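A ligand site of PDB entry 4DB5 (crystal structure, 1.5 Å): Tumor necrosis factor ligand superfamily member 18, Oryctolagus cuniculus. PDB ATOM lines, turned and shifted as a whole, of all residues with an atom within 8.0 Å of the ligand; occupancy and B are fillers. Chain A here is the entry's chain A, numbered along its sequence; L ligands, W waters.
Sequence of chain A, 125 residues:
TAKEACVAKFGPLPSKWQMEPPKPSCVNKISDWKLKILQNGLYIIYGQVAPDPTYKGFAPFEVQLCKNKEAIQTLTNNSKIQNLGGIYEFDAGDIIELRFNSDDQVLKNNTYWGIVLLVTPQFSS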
ATOM      1  N   SER A  25     -10.775  26.502  -8.850  1.00  0.00           N
ATOM      2  CA  SER A  25     -10.751  25.455  -9.839  1.00  0.00           C
ATOM      3  C   SER A  25      -9.974  24.243  -9.339  1.00  0.00           C
ATOM      4  O   SER A  25     -10.219  23.123  -9.786  1.00  0.00           O
ATOM      5  CB  SER A  25     -10.105  25.964 -11.134  1.00  0.00           C
ATOM      6  OG  SER A  25      -8.719  26.219 -10.955  1.00  0.00           O
ATOM      7  N   CYS A  26      -9.051  24.449  -8.408  1.00  0.00           N
ATOM      8  CA  CYS A  26      -8.074  23.413  -8.122  1.00  0.00           C
ATOM      9  C   CYS A  26      -8.482  22.435  -7.020  1.00  0.00           C
ATOM     10  O   CYS A  26      -8.023  21.292  -7.013  1.00  0.00           O
ATOM     11  CB  CYS A  26      -6.682  24.005  -7.851  1.00  0.00           C
ATOM     12  SG  CYS A  26      -6.411  24.739  -6.232  1.00  0.00           S
ATOM     13  N   ILE A  37      -8.670  17.187  -4.218  1.00  0.00           N
ATOM     14  CA  ILE A  37      -7.938  17.784  -5.336  1.00  0.00           C
ATOM     15  C   ILE A  37      -8.758  17.623  -6.600  1.00  0.00           C
ATOM     16  O   ILE A  37      -9.250  16.533  -6.897  1.00  0.00           O
ATOM     17  CB  ILE A  37      -6.587  17.082  -5.531  1.00  0.00           C
ATOM     18  CG1 ILE A  37      -5.722  17.159  -4.264  1.00  0.00           C
ATOM     19  CG2 ILE A  37      -5.848  17.652  -6.742  1.00  0.00           C
ATOM     20  CD1 ILE A  37      -5.365  18.584  -3.827  1.00  0.00           C
ATOM     21  N   LEU A  38      -8.931  18.716  -7.356  1.00  0.00           N
ATOM     22  CA  LEU A  38      -9.681  18.662  -8.617  1.00  0.00           C
ATOM     23  C   LEU A  38      -8.768  18.729  -9.830  1.00  0.00           C
ATOM     24  O   LEU A  38      -9.108  18.230 -10.900  1.00  0.00           O
ATOM     25  CB  LEU A  38     -10.696  19.823  -8.692  1.00  0.00           C
ATOM     26  CG  LEU A  38     -11.749  19.909  -7.596  1.00  0.00           C
ATOM     27  CD1 LEU A  38     -12.681  21.093  -7.885  1.00  0.00           C
ATOM     28  CD2 LEU A  38     -12.538  18.623  -7.520  1.00  0.00           C
ATOM     29  N   GLN A  39      -7.603  19.350  -9.666  1.00  0.00           N
ATOM     30  CA  GLN A  39      -6.706  19.605 -10.787  1.00  0.00           C
ATOM     31  C   GLN A  39      -5.387  18.870 -10.573  1.00  0.00           C
ATOM     32  O   GLN A  39      -4.752  19.030  -9.517  1.00  0.00           O
ATOM     33  CB  GLN A  39      -6.467  21.108 -10.904  1.00  0.00           C
ATOM     34  CG  GLN A  39      -6.079  21.607 -12.285  1.00  0.00           C
ATOM     35  CD  GLN A  39      -6.223  23.114 -12.392  1.00  0.00           C
ATOM     36  OE1 GLN A  39      -6.429  23.811 -11.384  1.00  0.00           O
ATOM     37  NE2 GLN A  39      -6.140  23.636 -13.610  1.00  0.00           N
ATOM     38  N   ASN A  40      -4.964  18.057 -11.531  1.00  0.00           N
ATOM     39  CA  ASN A  40      -3.651  17.427 -11.433  1.00  0.00           C
ATOM     40  C   ASN A  40      -2.575  18.491 -11.438  1.00  0.00           C
ATOM     41  O   ASN A  40      -2.639  19.457 -12.202  1.00  0.00           O
ATOM     42  CB  ASN A  40      -3.429  16.454 -12.587  1.00  0.00           C
ATOM     43  CG  ASN A  40      -4.293  15.241 -12.461  1.00  0.00           C
ATOM     44  OD1 ASN A  40      -5.498  15.360 -12.237  1.00  0.00           O
ATOM     45  ND2 ASN A  40      -3.687  14.062 -12.554  1.00  0.00           N
ATOM     46  N   GLY A  41      -1.596  18.345 -10.568  1.00  0.00           N
ATOM     47  CA  GLY A  41      -0.510  19.318 -10.561  1.00  0.00           C
ATOM     48  C   GLY A  41       0.375  19.216  -9.363  1.00  0.00           C
ATOM     49  O   GLY A  41       0.291  18.259  -8.596  1.00  0.00           O
ATOM     50  N   TYR A  43       1.483  20.827  -5.851  1.00  0.00           N
ATOM     51  CA  TYR A  43       0.910  21.615  -4.764  1.00  0.00           C
ATOM     52  C   TYR A  43       1.896  21.759  -3.623  1.00  0.00           C
ATOM     53  O   TYR A  43       2.632  20.816  -3.289  1.00  0.00           O
ATOM     54  CB  TYR A  43      -0.326  20.892  -4.226  1.00  0.00           C
ATOM     55  CG  TYR A  43      -1.488  20.902  -5.180  1.00  0.00           C
ATOM     56  CD1 TYR A  43      -1.615  19.925  -6.176  1.00  0.00           C
ATOM     57  CD2 TYR A  43      -2.475  21.875  -5.101  1.00  0.00           C
ATOM     58  CE1 TYR A  43      -2.695  19.938  -7.060  1.00  0.00           C
ATOM     59  CE2 TYR A  43      -3.550  21.897  -5.963  1.00  0.00           C
ATOM     60  CZ  TYR A  43      -3.654  20.927  -6.930  1.00  0.00           C
ATOM     61  OH  TYR A  43      -4.738  20.980  -7.794  1.00  0.00           O
ATOM     62  N   GLU A  89       3.038  16.078  -5.972  1.00  0.00           N
ATOM     63  CA  GLU A  89       2.228  15.915  -7.171  1.00  0.00           C
ATOM     64  C   GLU A  89       0.945  15.162  -6.818  1.00  0.00           C
ATOM     65  O   GLU A  89       1.000  14.027  -6.323  1.00  0.00           O
ATOM     66  CB  GLU A  89       3.016  15.173  -8.260  1.00  0.00           C
ATOM     67  CG  GLU A  89       2.309  15.140  -9.612  1.00  0.00           C
ATOM     68  CD  GLU A  89       3.194  14.583 -10.729  1.00  0.00           C
ATOM     69  OE1 GLU A  89       4.395  14.929 -10.767  1.00  0.00           O
ATOM     70  OE2 GLU A  89       2.692  13.815 -11.561  1.00  0.00           O
ATOM     71  N   PHE A  90      -0.204  15.795  -7.030  1.00  0.00           N
ATOM     72  CA  PHE A  90      -1.492  15.155  -6.730  1.00  0.00           C
ATOM     73  C   PHE A  90      -2.316  14.935  -7.997  1.00  0.00           C
ATOM     74  O   PHE A  90      -2.127  15.613  -9.019  1.00  0.00           O
ATOM     75  CB  PHE A  90      -2.317  15.983  -5.736  1.00  0.00           C
ATOM     76  CG  PHE A  90      -1.747  16.044  -4.345  1.00  0.00           C
ATOM     77  CD1 PHE A  90      -1.184  14.911  -3.724  1.00  0.00           C
ATOM     78  CD2 PHE A  90      -1.798  17.223  -3.626  1.00  0.00           C
ATOM     79  CE1 PHE A  90      -0.679  15.000  -2.417  1.00  0.00           C
ATOM     80  CE2 PHE A  90      -1.300  17.313  -2.332  1.00  0.00           C
ATOM     81  CZ  PHE A  90      -0.742  16.201  -1.723  1.00  0.00           C
ATOM     82  N   ASP A  91      -3.230  13.968  -7.916  1.00  0.00           N
ATOM     83  CA  ASP A  91      -4.141  13.657  -9.002  1.00  0.00           C
ATOM     84  C   ASP A  91      -5.539  14.123  -8.626  1.00  0.00           C
ATOM     85  O   ASP A  91      -5.904  14.153  -7.450  1.00  0.00           O
ATOM     86  CB  ASP A  91      -4.173  12.143  -9.227  1.00  0.00           C
ATOM     87  CG  ASP A  91      -2.820  11.569  -9.621  1.00  0.00           C
ATOM     88  OD1 ASP A  91      -2.103  12.215 -10.426  1.00  0.00           O
ATOM     89  OD2 ASP A  91      -2.466  10.485  -9.121  1.00  0.00           O
ATOM     90  N   ALA A  92      -6.338  14.464  -9.643  1.00  0.00           N
ATOM     91  CA  ALA A  92      -7.744  14.767  -9.440  1.00  0.00           C
ATOM     92  C   ALA A  92      -8.388  13.589  -8.725  1.00  0.00           C
ATOM     93  O   ALA A  92      -8.194  12.427  -9.101  1.00  0.00           O
ATOM     94  CB  ALA A  92      -8.443  15.014 -10.785  1.00  0.00           C
ATOM     95  N   GLY A  93      -9.128  13.887  -7.659  1.00  0.00           N
ATOM     96  CA  GLY A  93      -9.803  12.868  -6.877  1.00  0.00           C
ATOM     97  C   GLY A  93      -9.074  12.551  -5.577  1.00  0.00           C
ATOM     98  O   GLY A  93      -9.648  11.942  -4.681  1.00  0.00           O
ATOM     99  N   ASP A  94      -7.802  12.956  -5.465  1.00  0.00           N
ATOM    100  CA  ASP A  94      -7.082  12.702  -4.219  1.00  0.00           C
ATOM    101  C   ASP A  94      -7.724  13.452  -3.060  1.00  0.00           C
ATOM    102  O   ASP A  94      -8.073  14.622  -3.167  1.00  0.00           O
ATOM    103  CB  ASP A  94      -5.610  13.123  -4.325  1.00  0.00           C
ATOM    104  CG  ASP A  94      -4.766  12.146  -5.125  1.00  0.00           C
ATOM    105  OD1 ASP A  94      -5.190  10.989  -5.359  1.00  0.00           O
ATOM    106  OD2 ASP A  94      -3.652  12.551  -5.529  1.00  0.00           O
ATOM    107  N   THR A 120       0.681  23.397 -13.060  1.00  0.00           N
ATOM    108  CA  THR A 120      -0.130  22.286 -13.579  1.00  0.00           C
ATOM    109  C   THR A 120       0.510  21.670 -14.831  1.00  0.00           C
ATOM    110  O   THR A 120       0.006  21.875 -15.943  1.00  0.00           O
ATOM    111  CB  THR A 120      -1.569  22.742 -13.911  1.00  0.00           C
ATOM    112  OG1 THR A 120      -1.516  23.865 -14.802  1.00  0.00           O
ATOM    113  CG2 THR A 120      -2.317  23.123 -12.646  1.00  0.00           C
ATOM    114  N   PRO A 121       1.613  20.921 -14.667  1.00  0.00           N
ATOM    115  CA  PRO A 121       2.334  20.367 -15.828  1.00  0.00           C
ATOM    116  C   PRO A 121       1.510  19.314 -16.551  1.00  0.00           C
ATOM    117  O   PRO A 121       0.700  18.610 -15.925  1.00  0.00           O
ATOM    118  CB  PRO A 121       3.564  19.702 -15.200  1.00  0.00           C
ATOM    119  CG  PRO A 121       3.652  20.246 -13.803  1.00  0.00           C
ATOM    120  CD  PRO A 121       2.228  20.502 -13.396  1.00  0.00           C
ATOM    121  N   GLN A 122       1.700  19.191 -17.859  1.00  0.00           N
ATOM    122  CA  GLN A 122       1.040  18.128 -18.601  1.00  0.00           C
ATOM    123  C   GLN A 122       1.441  16.758 -18.059  1.00  0.00           C
ATOM    124  O   GLN A 122       0.631  15.826 -18.027  1.00  0.00           O
ATOM    125  CB  GLN A 122       1.359  18.244 -20.085  1.00  0.00           C
ATOM    126  CG  GLN A 122       0.888  19.541 -20.693  1.00  0.00           C
ATOM    127  CD  GLN A 122       1.270  19.641 -22.146  1.00  0.00           C
ATOM    128  OE1 GLN A 122       2.424  19.871 -22.486  1.00  0.00           O
ATOM    129  NE2 GLN A 122       0.290  19.427 -23.032  1.00  0.00           N
ATOM    130  N   PHE A 123       2.684  16.641 -17.596  1.00  0.00           N
ATOM    131  CA  PHE A 123       3.158  15.358 -17.092  1.00  0.00           C
ATOM    132  C   PHE A 123       2.539  14.916 -15.766  1.00  0.00           C
ATOM    133  O   PHE A 123       2.775  13.791 -15.306  1.00  0.00           O
ATOM    134  CB  PHE A 123       4.700  15.287 -17.045  1.00  0.00           C
ATOM    135  CG  PHE A 123       5.367  16.302 -16.112  1.00  0.00           C
ATOM    136  CD1 PHE A 123       5.065  16.360 -14.768  1.00  0.00           C
ATOM    137  CD2 PHE A 123       6.385  17.127 -16.604  1.00  0.00           C
ATOM    138  CE1 PHE A 123       5.695  17.281 -13.933  1.00  0.00           C
ATOM    139  CE2 PHE A 123       7.029  18.026 -15.754  1.00  0.00           C
ATOM    140  CZ  PHE A 123       6.683  18.099 -14.435  1.00  0.00           C
ATOM    141  N   SER A 124       1.751  15.786 -15.159  1.00  0.00           N
ATOM    142  CA  SER A 124       1.126  15.468 -13.886  1.00  0.00           C
ATOM    143  C   SER A 124      -0.173  14.696 -14.066  1.00  0.00           C
ATOM    144  O   SER A 124      -0.783  14.267 -13.084  1.00  0.00           O
ATOM    145  CB  SER A 124       0.893  16.724 -13.047  1.00  0.00           C
ATOM    146  OG  SER A 124       2.117  17.313 -12.652  1.00  0.00           O
ATOM    147  N   SER A 125      -0.588  14.509 -15.313  1.00  0.00           N
ATOM    148  CA  SER A 125      -1.784  13.725 -15.616  1.00  0.00           C
ATOM    149  C   SER A 125      -1.519  12.675 -16.694  1.00  0.00           C
ATOM    150  O   SER A 125      -0.668  12.854 -17.568  1.00  0.00           O
ATOM    151  CB  SER A 125      -2.945  14.618 -16.050  1.00  0.00           C
ATOM    152  OG  SER A 125      -2.825  14.983 -17.416  1.00  0.00           O
ATOM    153  OXT SER A 125      -2.166  11.634 -16.705  1.00  0.00           O
HETATM  154  C1  LIG L   1      -7.374  13.832 -14.233  1.00  0.00           C
HETATM  155  C2  LIG L   1      -6.493  12.680 -14.708  1.00  0.00           C
HETATM  156  C3  LIG L   1      -7.162  15.064 -15.101  1.00  0.00           C
HETATM  157  N1  LIG L   1      -7.789  16.267 -14.551  1.00  0.00           N
HETATM  158  C4  LIG L   1      -7.835  17.483 -15.347  1.00  0.00           C
HETATM  159  C5  LIG L   1      -8.738  18.467 -14.619  1.00  0.00           C
HETATM  160  C6  LIG L   1      -6.421  18.041 -15.533  1.00  0.00           C
HETATM  161  C7  LIG L   1      -8.468  17.164 -16.700  1.00  0.00           C
HETATM  162  N2  LIG L   1      -6.550  11.498 -13.850  1.00  0.00           N
HETATM  163  C8  LIG L   1      -6.092  10.214 -14.352  1.00  0.00           C
HETATM  164  C9  LIG L   1      -7.219   9.586 -15.178  1.00  0.00           C
HETATM  165  C10 LIG L   1      -5.710   9.303 -13.197  1.00  0.00           C
HETATM  166  C11 LIG L   1      -4.857  10.398 -15.236  1.00  0.00           C
HETATM  167  O1  LIG L   1      -8.477   9.802 -14.517  1.00  0.00           O
HETATM  168  O2  LIG L   1      -6.731   9.281 -12.187  1.00  0.00           O
HETATM  169  O3  LIG L   1      -3.840  11.108 -14.507  1.00  0.00           O
HETATM  170  O4  LIG L   1      -8.415  19.823 -14.963  1.00  0.00           O
HETATM  171  O5  LIG L   1      -5.869  18.429 -14.269  1.00  0.00           O
HETATM  172  O6  LIG L   1      -7.501  17.082 -17.761  1.00  0.00           O
HETATM  173  O   HOH W   1      -2.175  10.482 -12.723  1.00  0.00           O
HETATM  174  O   HOH W   2     -10.495  15.745 -13.897  1.00  0.00           O
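OD1 of Asn 40 sits close to N1 of the ligand (3.4 Å). O3 of the ligand sits at hydrogen-bond distance from OXT of Ser 125 (2.8 Å). O5 of the ligand sits at hydrogen-bond distance from N of Asn 40 (2.9 Å).
N of Gln 39 is in hydrogen-bond range of O of Cys 26, at 3.3 Å. OH of Tyr 43 sits at hydrogen-bond distance from O of Gln 39, 2.6 Å away. N of Ala 92 sits at hydrogen-bond distance from OD1 of Asn 40 (2.9 Å). The backbone carbonyl oxygen (O) of Ser 124 is in hydrogen-bond range of the side-chain amide nitrogen (ND2) of Asn 40. The side-chain carboxylate of Asp 91 lies within hydrogen-bond range of the side-chain amide nitrogen of Asn 40 (3.2 Å). The backbone NH (N) of Leu 38 sits at hydrogen-bond distance from the backbone carbonyl oxygen (O) of Cys 26 (2.8 Å). The side-chain hydroxyl of Ser 25 lies within hydrogen-bond range of the side-chain amide oxygen of Gln 39.
Merely in contact with the ligand: Leu 38 (3.7 Å), Gln 39 (3.8 Å) and Ala 92 (3.8 Å). Hydrophobic or aromatic side chains within 4 Å of the ligand: Ala 92. Five residues have an atom within 4 Å of the ligand: Leu 38, Gln 39, Asn 40, Ala 92 and Ser 125.
Water W1 lies within hydrogen-bond range of O3 of the ligand (2.5 Å) and OD1 of Asp 91 (2.9 Å).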
